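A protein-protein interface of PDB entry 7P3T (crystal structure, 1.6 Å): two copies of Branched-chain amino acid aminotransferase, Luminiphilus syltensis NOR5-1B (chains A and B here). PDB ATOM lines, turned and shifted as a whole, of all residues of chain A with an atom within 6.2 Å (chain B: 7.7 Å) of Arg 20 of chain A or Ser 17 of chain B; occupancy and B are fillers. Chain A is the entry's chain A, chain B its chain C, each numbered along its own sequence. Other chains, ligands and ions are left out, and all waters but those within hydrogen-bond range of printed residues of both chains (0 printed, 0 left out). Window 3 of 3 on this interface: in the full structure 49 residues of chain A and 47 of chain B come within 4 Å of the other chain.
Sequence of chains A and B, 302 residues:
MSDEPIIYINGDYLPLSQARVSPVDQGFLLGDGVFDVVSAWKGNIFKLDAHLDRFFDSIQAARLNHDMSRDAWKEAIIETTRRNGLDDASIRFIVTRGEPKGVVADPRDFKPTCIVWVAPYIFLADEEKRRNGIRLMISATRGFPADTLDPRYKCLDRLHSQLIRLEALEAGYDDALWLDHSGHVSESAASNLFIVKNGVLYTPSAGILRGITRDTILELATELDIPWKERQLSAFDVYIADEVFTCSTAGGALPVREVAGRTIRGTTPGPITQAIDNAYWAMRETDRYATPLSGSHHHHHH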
ATOM      1  N   ILE A   7      -6.204 -15.440  32.355  1.00  0.00           N
ATOM      2  CA  ILE A   7      -6.849 -16.698  32.698  1.00  0.00           C
ATOM      3  C   ILE A   7      -6.786 -17.650  31.509  1.00  0.00           C
ATOM      4  O   ILE A   7      -6.576 -17.251  30.360  1.00  0.00           O
ATOM      5  CB  ILE A   7      -8.301 -16.534  33.177  1.00  0.00           C
ATOM      6  CG1 ILE A   7      -9.212 -16.198  32.023  1.00  0.00           C
ATOM      7  CG2 ILE A   7      -8.437 -15.483  34.285  1.00  0.00           C
ATOM      8  CD1 ILE A   7     -10.602 -16.621  32.288  1.00  0.00           C
ATOM      9  N   ILE A   9      -9.210 -20.134  29.453  1.00  0.00           N
ATOM     10  CA  ILE A   9     -10.617 -20.432  29.207  1.00  0.00           C
ATOM     11  C   ILE A   9     -10.732 -21.166  27.875  1.00  0.00           C
ATOM     12  O   ILE A   9     -10.378 -20.649  26.794  1.00  0.00           O
ATOM     13  CB  ILE A   9     -11.508 -19.173  29.289  1.00  0.00           C
ATOM     14  CG1 ILE A   9     -12.981 -19.556  29.083  1.00  0.00           C
ATOM     15  CG2 ILE A   9     -11.080 -18.098  28.311  1.00  0.00           C
ATOM     16  CD1 ILE A   9     -13.927 -18.511  29.544  1.00  0.00           C
ATOM     17  N   ASN A  10     -11.168 -22.430  27.961  1.00  0.00           N
ATOM     18  CA  ASN A  10     -11.395 -23.276  26.799  1.00  0.00           C
ATOM     19  C   ASN A  10     -10.215 -23.274  25.828  1.00  0.00           C
ATOM     20  O   ASN A  10     -10.387 -23.232  24.614  1.00  0.00           O
ATOM     21  CB  ASN A  10     -12.673 -22.851  26.088  1.00  0.00           C
ATOM     22  CG  ASN A  10     -13.885 -22.942  26.968  1.00  0.00           C
ATOM     23  OD1 ASN A  10     -13.929 -23.746  27.891  1.00  0.00           O
ATOM     24  ND2 ASN A  10     -14.868 -22.079  26.716  1.00  0.00           N
ATOM     25  N   LEU A  14      -6.013 -15.470  27.996  1.00  0.00           N
ATOM     26  CA  LEU A  14      -6.249 -14.060  27.707  1.00  0.00           C
ATOM     27  C   LEU A  14      -6.557 -13.311  29.001  1.00  0.00           C
ATOM     28  O   LEU A  14      -6.807 -13.915  30.031  1.00  0.00           O
ATOM     29  CB  LEU A  14      -7.376 -13.873  26.695  1.00  0.00           C
ATOM     30  CG  LEU A  14      -8.797 -14.126  27.162  1.00  0.00           C
ATOM     31  CD1 LEU A  14      -9.755 -13.817  26.000  1.00  0.00           C
ATOM     32  CD2 LEU A  14      -8.974 -15.533  27.628  1.00  0.00           C
ATOM     33  N   LEU A  16      -8.319 -11.415  31.977  1.00  0.00           N
ATOM     34  CA  LEU A  16      -9.625 -11.624  32.598  1.00  0.00           C
ATOM     35  C   LEU A  16     -10.641 -10.638  32.045  1.00  0.00           C
ATOM     36  O   LEU A  16     -11.806 -10.998  31.817  1.00  0.00           O
ATOM     37  CB  LEU A  16      -9.497 -11.465  34.111  1.00  0.00           C
ATOM     38  CG  LEU A  16     -10.763 -11.521  34.970  1.00  0.00           C
ATOM     39  CD1 LEU A  16     -11.476 -12.819  34.829  1.00  0.00           C
ATOM     40  CD2 LEU A  16     -10.400 -11.267  36.442  1.00  0.00           C
ATOM     41  N   GLN A  18     -11.136  -9.556  29.217  1.00  0.00           N
ATOM     42  CA  GLN A  18     -11.624  -9.931  27.900  1.00  0.00           C
ATOM     43  C   GLN A  18     -12.271 -11.303  27.900  1.00  0.00           C
ATOM     44  O   GLN A  18     -13.117 -11.592  27.050  1.00  0.00           O
ATOM     45  CB  GLN A  18     -10.466  -9.921  26.901  1.00  0.00           C
ATOM     46  CG  GLN A  18      -9.850  -8.546  26.644  1.00  0.00           C
ATOM     47  CD  GLN A  18     -10.876  -7.543  26.148  1.00  0.00           C
ATOM     48  OE1 GLN A  18     -11.638  -7.819  25.220  1.00  0.00           O
ATOM     49  NE2 GLN A  18     -10.908  -6.379  26.773  1.00  0.00           N
ATOM     50  N   ALA A  19     -11.886 -12.152  28.846  1.00  0.00           N
ATOM     51  CA  ALA A  19     -12.427 -13.495  28.923  1.00  0.00           C
ATOM     52  C   ALA A  19     -13.928 -13.464  29.210  1.00  0.00           C
ATOM     53  O   ALA A  19     -14.410 -12.650  29.996  1.00  0.00           O
ATOM     54  CB  ALA A  19     -11.706 -14.278  30.011  1.00  0.00           C
ATOM     55  N   ARG A  20     -14.658 -14.376  28.571  1.00  0.00           N
ATOM     56  CA  ARG A  20     -16.115 -14.321  28.530  1.00  0.00           C
ATOM     57  C   ARG A  20     -16.716 -15.658  28.927  1.00  0.00           C
ATOM     58  O   ARG A  20     -16.441 -16.689  28.289  1.00  0.00           O
ATOM     59  CB  ARG A  20     -16.627 -13.942  27.137  1.00  0.00           C
ATOM     60  CG  ARG A  20     -18.126 -14.205  26.926  1.00  0.00           C
ATOM     61  CD  ARG A  20     -18.566 -13.769  25.531  1.00  0.00           C
ATOM     62  NE  ARG A  20     -19.976 -14.068  25.281  1.00  0.00           N
ATOM     63  CZ  ARG A  20     -20.430 -15.230  24.829  1.00  0.00           C
ATOM     64  NH1 ARG A  20     -21.724 -15.393  24.609  1.00  0.00           N
ATOM     65  NH2 ARG A  20     -19.591 -16.218  24.551  1.00  0.00           N
ATOM     66  N   VAL A  21     -17.574 -15.617  29.928  1.00  0.00           N
ATOM     67  CA  VAL A  21     -18.562 -16.655  30.178  1.00  0.00           C
ATOM     68  C   VAL A  21     -19.861 -16.184  29.542  1.00  0.00           C
ATOM     69  O   VAL A  21     -20.258 -15.021  29.702  1.00  0.00           O
ATOM     70  CB  VAL A  21     -18.744 -16.904  31.681  1.00  0.00           C
ATOM     71  CG1 VAL A  21     -19.925 -17.846  31.934  1.00  0.00           C
ATOM     72  CG2 VAL A  21     -17.477 -17.496  32.298  1.00  0.00           C
ATOM     73  N   SER A  22     -20.505 -17.060  28.800  1.00  0.00           N
ATOM     74  CA  SER A  22     -21.768 -16.690  28.182  1.00  0.00           C
ATOM     75  C   SER A  22     -22.843 -16.516  29.249  1.00  0.00           C
ATOM     76  O   SER A  22     -22.928 -17.326  30.172  1.00  0.00           O
ATOM     77  CB  SER A  22     -22.226 -17.764  27.213  1.00  0.00           C
ATOM     78  OG  SER A  22     -23.561 -17.512  26.800  1.00  0.00           O
ATOM     79  N   PRO A  23     -23.736 -15.534  29.096  1.00  0.00           N
ATOM     80  CA  PRO A  23     -24.876 -15.432  30.012  1.00  0.00           C
ATOM     81  C   PRO A  23     -25.772 -16.648  29.990  1.00  0.00           C
ATOM     82  O   PRO A  23     -26.596 -16.787  30.893  1.00  0.00           O
ATOM     83  CB  PRO A  23     -25.633 -14.189  29.529  1.00  0.00           C
ATOM     84  CG  PRO A  23     -24.794 -13.537  28.544  1.00  0.00           C
ATOM     85  CD  PRO A  23     -23.707 -14.453  28.096  1.00  0.00           C
ATOM     86  N   GLU A  99     -22.583 -24.210  27.451  1.00  0.00           N
ATOM     87  CA  GLU A  99     -23.716 -23.587  26.809  1.00  0.00           C
ATOM     88  C   GLU A  99     -24.604 -24.652  26.176  1.00  0.00           C
ATOM     89  O   GLU A  99     -24.117 -25.719  25.787  1.00  0.00           O
ATOM     90  CB  GLU A  99     -23.244 -22.577  25.752  1.00  0.00           C
ATOM     91  CG  GLU A  99     -22.408 -21.441  26.374  1.00  0.00           C
ATOM     92  CD  GLU A  99     -21.454 -20.758  25.394  1.00  0.00           C
ATOM     93  OE1 GLU A  99     -20.318 -20.407  25.795  1.00  0.00           O
ATOM     94  OE2 GLU A  99     -21.847 -20.565  24.238  1.00  0.00           O
ATOM     95  N   THR A 113     -17.336 -25.802  29.696  1.00  0.00           N
ATOM     96  CA  THR A 113     -16.540 -24.595  29.903  1.00  0.00           C
ATOM     97  C   THR A 113     -15.454 -24.947  30.906  1.00  0.00           C
ATOM     98  O   THR A 113     -15.766 -25.438  31.988  1.00  0.00           O
ATOM     99  CB  THR A 113     -17.410 -23.461  30.422  1.00  0.00           C
ATOM    100  OG1 THR A 113     -18.371 -23.125  29.408  1.00  0.00           O
ATOM    101  CG2 THR A 113     -16.565 -22.234  30.750  1.00  0.00           C
ATOM    102  N   GLU B   4     -28.930 -13.477  15.884  1.00  0.00           N
ATOM    103  CA  GLU B   4     -28.676 -14.016  17.201  1.00  0.00           C
ATOM    104  C   GLU B   4     -29.440 -13.242  18.269  1.00  0.00           C
ATOM    105  O   GLU B   4     -29.856 -12.099  18.064  1.00  0.00           O
ATOM    106  CB  GLU B   4     -27.177 -14.024  17.505  1.00  0.00           C
ATOM    107  CG  GLU B   4     -26.503 -12.687  17.688  1.00  0.00           C
ATOM    108  CD  GLU B   4     -25.058 -12.842  18.153  1.00  0.00           C
ATOM    109  OE1 GLU B   4     -24.824 -13.514  19.179  1.00  0.00           O
ATOM    110  OE2 GLU B   4     -24.157 -12.299  17.484  1.00  0.00           O
ATOM    111  N   PRO B   5     -29.662 -13.868  19.414  1.00  0.00           N
ATOM    112  CA  PRO B   5     -30.380 -13.186  20.495  1.00  0.00           C
ATOM    113  C   PRO B   5     -29.697 -11.902  20.925  1.00  0.00           C
ATOM    114  O   PRO B   5     -28.465 -11.774  20.897  1.00  0.00           O
ATOM    115  CB  PRO B   5     -30.372 -14.216  21.630  1.00  0.00           C
ATOM    116  CG  PRO B   5     -30.167 -15.538  20.955  1.00  0.00           C
ATOM    117  CD  PRO B   5     -29.270 -15.241  19.789  1.00  0.00           C
ATOM    118  N   ILE B   6     -30.521 -10.950  21.359  1.00  0.00           N
ATOM    119  CA  ILE B   6     -30.053  -9.720  21.976  1.00  0.00           C
ATOM    120  C   ILE B   6     -30.296  -9.820  23.481  1.00  0.00           C
ATOM    121  O   ILE B   6     -31.404 -10.152  23.922  1.00  0.00           O
ATOM    122  CB  ILE B   6     -30.753  -8.488  21.374  1.00  0.00           C
ATOM    123  CG1 ILE B   6     -30.437  -8.327  19.881  1.00  0.00           C
ATOM    124  CG2 ILE B   6     -30.336  -7.257  22.170  1.00  0.00           C
ATOM    125  CD1 ILE B   6     -29.001  -8.060  19.614  1.00  0.00           C
ATOM    126  N   ILE B   7     -29.253  -9.559  24.267  1.00  0.00           N
ATOM    127  CA  ILE B   7     -29.272  -9.700  25.721  1.00  0.00           C
ATOM    128  C   ILE B   7     -29.195  -8.314  26.338  1.00  0.00           C
ATOM    129  O   ILE B   7     -28.428  -7.466  25.865  1.00  0.00           O
ATOM    130  CB  ILE B   7     -28.074 -10.543  26.202  1.00  0.00           C
ATOM    131  CG1 ILE B   7     -28.046 -11.931  25.568  1.00  0.00           C
ATOM    132  CG2 ILE B   7     -28.035 -10.644  27.723  1.00  0.00           C
ATOM    133  CD1 ILE B   7     -29.161 -12.840  25.972  1.00  0.00           C
ATOM    134  N   LEU B  14     -26.952  -6.083  23.838  1.00  0.00           N
ATOM    135  CA  LEU B  14     -25.849  -6.627  23.069  1.00  0.00           C
ATOM    136  C   LEU B  14     -26.212  -7.977  22.477  1.00  0.00           C
ATOM    137  O   LEU B  14     -26.933  -8.763  23.101  1.00  0.00           O
ATOM    138  CB  LEU B  14     -24.609  -6.795  23.956  1.00  0.00           C
ATOM    139  CG  LEU B  14     -24.002  -5.533  24.563  1.00  0.00           C
ATOM    140  CD1 LEU B  14     -22.928  -5.925  25.559  1.00  0.00           C
ATOM    141  CD2 LEU B  14     -23.439  -4.665  23.446  1.00  0.00           C
ATOM    142  N   PRO B  15     -25.709  -8.283  21.291  1.00  0.00           N
ATOM    143  CA  PRO B  15     -25.810  -9.657  20.785  1.00  0.00           C
ATOM    144  C   PRO B  15     -25.183 -10.634  21.763  1.00  0.00           C
ATOM    145  O   PRO B  15     -24.174 -10.338  22.408  1.00  0.00           O
ATOM    146  CB  PRO B  15     -25.035  -9.616  19.466  1.00  0.00           C
ATOM    147  CG  PRO B  15     -25.001  -8.203  19.074  1.00  0.00           C
ATOM    148  CD  PRO B  15     -25.029  -7.396  20.317  1.00  0.00           C
ATOM    149  N   LEU B  16     -25.784 -11.819  21.851  1.00  0.00           N
ATOM    150  CA  LEU B  16     -25.350 -12.790  22.855  1.00  0.00           C
ATOM    151  C   LEU B  16     -23.857 -13.066  22.756  1.00  0.00           C
ATOM    152  O   LEU B  16     -23.162 -13.121  23.774  1.00  0.00           O
ATOM    153  CB  LEU B  16     -26.139 -14.087  22.683  1.00  0.00           C
ATOM    154  CG  LEU B  16     -25.736 -15.276  23.570  1.00  0.00           C
ATOM    155  CD1 LEU B  16     -25.992 -14.986  25.030  1.00  0.00           C
ATOM    156  CD2 LEU B  16     -26.480 -16.508  23.094  1.00  0.00           C
ATOM    157  N   SER B  17     -23.348 -13.232  21.537  1.00  0.00           N
ATOM    158  CA  SER B  17     -21.936 -13.530  21.332  1.00  0.00           C
ATOM    159  C   SER B  17     -21.023 -12.469  21.922  1.00  0.00           C
ATOM    160  O   SER B  17     -19.849 -12.757  22.186  1.00  0.00           O
ATOM    161  CB  SER B  17     -21.644 -13.661  19.841  1.00  0.00           C
ATOM    162  OG  SER B  17     -21.934 -12.456  19.139  1.00  0.00           O
ATOM    163  N   GLN B  18     -21.514 -11.246  22.088  1.00  0.00           N
ATOM    164  CA  GLN B  18     -20.725 -10.158  22.646  1.00  0.00           C
ATOM    165  C   GLN B  18     -20.973  -9.942  24.131  1.00  0.00           C
ATOM    166  O   GLN B  18     -20.116  -9.374  24.813  1.00  0.00           O
ATOM    167  CB  GLN B  18     -21.025  -8.853  21.899  1.00  0.00           C
ATOM    168  CG  GLN B  18     -20.522  -8.830  20.453  1.00  0.00           C
ATOM    169  CD  GLN B  18     -21.090  -7.672  19.652  1.00  0.00           C
ATOM    170  OE1 GLN B  18     -21.372  -7.807  18.458  1.00  0.00           O
ATOM    171  NE2 GLN B  18     -21.264  -6.527  20.304  1.00  0.00           N
ATOM    172  N   ALA B  19     -22.122 -10.377  24.634  1.00  0.00           N
ATOM    173  CA  ALA B  19     -22.494 -10.184  26.029  1.00  0.00           C
ATOM    174  C   ALA B  19     -21.618 -11.050  26.913  1.00  0.00           C
ATOM    175  O   ALA B  19     -21.386 -12.224  26.609  1.00  0.00           O
ATOM    176  CB  ALA B  19     -23.961 -10.544  26.225  1.00  0.00           C
ATOM    177  N   ARG B  20     -21.080 -10.451  27.966  1.00  0.00           N
ATOM    178  CA  ARG B  20     -20.058 -11.106  28.768  1.00  0.00           C
ATOM    179  C   ARG B  20     -20.429 -11.121  30.239  1.00  0.00           C
ATOM    180  O   ARG B  20     -20.665 -10.067  30.841  1.00  0.00           O
ATOM    181  CB  ARG B  20     -18.716 -10.406  28.618  1.00  0.00           C
ATOM    182  CG  ARG B  20     -17.653 -10.825  29.616  1.00  0.00           C
ATOM    183  CD  ARG B  20     -16.420  -9.994  29.421  1.00  0.00           C
ATOM    184  NE  ARG B  20     -15.410 -10.227  30.436  1.00  0.00           N
ATOM    185  CZ  ARG B  20     -15.315  -9.550  31.572  1.00  0.00           C
ATOM    186  NH1 ARG B  20     -14.337  -9.826  32.414  1.00  0.00           N
ATOM    187  NH2 ARG B  20     -16.184  -8.584  31.849  1.00  0.00           N
ATOM    188  N   VAL B  21     -20.403 -12.314  30.821  1.00  0.00           N
ATOM    189  CA  VAL B  21     -20.304 -12.490  32.265  1.00  0.00           C
ATOM    190  C   VAL B  21     -18.836 -12.689  32.596  1.00  0.00           C
ATOM    191  O   VAL B  21     -18.137 -13.463  31.931  1.00  0.00           O
ATOM    192  CB  VAL B  21     -21.165 -13.674  32.733  1.00  0.00           C
ATOM    193  CG1 VAL B  21     -20.995 -13.907  34.231  1.00  0.00           C
ATOM    194  CG2 VAL B  21     -22.644 -13.394  32.399  1.00  0.00           C
ATOM    195  N   SER B  22     -18.337 -11.964  33.587  1.00  0.00           N
ATOM    196  CA  SER B  22     -16.954 -12.151  33.968  1.00  0.00           C
ATOM    197  C   SER B  22     -16.754 -13.547  34.557  1.00  0.00           C
ATOM    198  O   SER B  22     -17.610 -14.020  35.310  1.00  0.00           O
ATOM    199  CB  SER B  22     -16.535 -11.128  35.014  1.00  0.00           C
ATOM    200  OG  SER B  22     -15.270 -11.458  35.498  1.00  0.00           O
ATOM    201  N   PRO B  23     -15.626 -14.207  34.268  1.00  0.00           N
ATOM    202  CA  PRO B  23     -15.327 -15.472  34.966  1.00  0.00           C
ATOM    203  C   PRO B  23     -15.276 -15.338  36.476  1.00  0.00           C
ATOM    204  O   PRO B  23     -15.364 -16.361  37.172  1.00  0.00           O
ATOM    205  CB  PRO B  23     -13.963 -15.879  34.395  1.00  0.00           C
ATOM    206  CG  PRO B  23     -13.924 -15.252  33.043  1.00  0.00           C
ATOM    207  CD  PRO B  23     -14.665 -13.937  33.185  1.00  0.00           C
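Printed residues of chain B that touch a printed residue of chain A: Leu 16, Ser 17, Ala 19, Arg 20, Val 21 and Pro 23.
Hydrophobic or aromatic side chains of chain B that line the printed part of chain A: Leu 16, Ala 19, Val 21 and Pro 23.
Printed residues of chain A that touch a printed residue of chain B: Ile 7, Leu 16, Ala 19, Arg 20, Val 21, Ser 22 and Pro 23.
Hydrophobic or aromatic side chains of chain A that line the printed part of chain B: Ile 7, Leu 16, Ala 19, Val 21 and Pro 23.
The backbone NH of Leu 16 of chain B sits at hydrogen-bond distance from the backbone carbonyl oxygen of Pro 5 of chain B (2.8 Å).
The side-chain carboxylate (OE2) of Glu 4 of chain B lies within hydrogen-bond range of the side-chain hydroxyl (OG) of Ser 17 of chain B (2.8 Å).
N of Ile 7 of chain A sits at hydrogen-bond distance from O of Leu 14 of chain A (2.8 Å).
N of Leu 16 of chain B is in hydrogen-bond range of OE1 of Glu 4 of chain B (3.3 Å).
CD1 of Ile 7 of chain A touches CG of Pro 23 of chain B, at 3.7 Å.
Pro 23 of chain B touches Leu 16 of chain A (CD to CD1, 3.8 Å).
Pro 23 of chain B touches Ala 19 of chain A (CD to O, 3.4 Å).
Arg 20 of chain A touches Arg 20 of chain B (CA to CG, 3.97 Å).
O of Val 21 of chain B touches C of Arg 20 of chain A, at 3.98 Å.
Arg 20 of chain B touches Val 21 of chain A (C to O, 3.9 Å).
Val 21 of chain A touches Pro 23 of chain B (CG2 to CA, 3.98 Å).
Pro 23 of chain A touches Leu 16 of chain B.
Pro 23 of chain A touches Ala 19 of chain B.
Pro 23 of chain A touches Val 21 of chain B.
The backbone carbonyl oxygen (O) of Val 21 of chain A is in hydrogen-bond range of the backbone NH (N) of Val 21 of chain B.
The guanidinium group (NH1) of Arg 20 of chain A is in hydrogen-bond range of the backbone carbonyl oxygen (O) of Leu 16 of chain B.
The guanidinium group (NE) of Arg 20 of chain A sits at hydrogen-bond distance from the backbone carbonyl oxygen (O) of Ala 19 of chain B.
The backbone carbonyl oxygen (O) of Ala 19 of chain A sits at hydrogen-bond distance from the guanidinium group (NE) of Arg 20 of chain B (2.7 Å).
The guanidinium group of Arg 20 of chain A lies within hydrogen-bond range of the backbone carbonyl oxygen of Ser 17 of chain B (3.4 Å).
The backbone carbonyl oxygen (O) of Leu 16 of chain A sits at hydrogen-bond distance from the guanidinium group (NH1) of Arg 20 of chain B (2.9 Å).
Of the printed residues of chain B, Leu 16 of chain A touches Arg 20 and Pro 23.
Ala 19 of chain A touches just these residues of chain B: Arg 20 (2.7 Å) and Pro 23 (3.4 Å).
Of the printed residues of chain B, Arg 20 of chain A touches Leu 16 (2.8 Å), Ser 17 (3.4 Å), Ala 19 (2.7 Å), Arg 20 (3.97 Å) and Val 21 (3.98 Å).
Of the printed residues of chain B, Val 21 of chain A touches Arg 20 (3.9 Å), Val 21 (2.9 Å) and Pro 23 (3.98 Å).
Ile 7 of chain B touches none of the printed residues of chain A.
Printed residues of chain A within 4 Å of Leu 16 of chain B: Arg 20 (2.8 Å), Ser 22 (3.9 Å) and Pro 23 (3.9 Å).
Of chain A, only Arg 20 comes within 4 Å of Ser 17 of chain B.
Of the printed residues of chain A, Ala 19 of chain B touches Arg 20 and Pro 23.
The nearest printed residue of chain B that does not touch Arg 20 of chain A is Gln 18 of chain B (4.4 Å).
The nearest printed residue of chain A that does not touch Ser 17 of chain B is Pro 23 of chain A (6.7 Å).
Leu 16 of chain A touches Pro 23 of chain B, and with the chains exchanged Pro 23 of chain A touches Leu 16 of chain B.
Ala 19 of chain A touches Arg 20 of chain B, and with the chains exchanged Arg 20 of chain A touches Ala 19 of chain B.
Ala 19 of chain A touches Pro 23 of chain B, and with the chains exchanged Pro 23 of chain A touches Ala 19 of chain B.
Val 21 of chain B touches its own counterpart, Val 21 of chain A.
9 positions are printed for both chains.
Of the 17 pairs that touch across the chains among the printed residues, 14 have their exchanged pair printed and touching as well.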
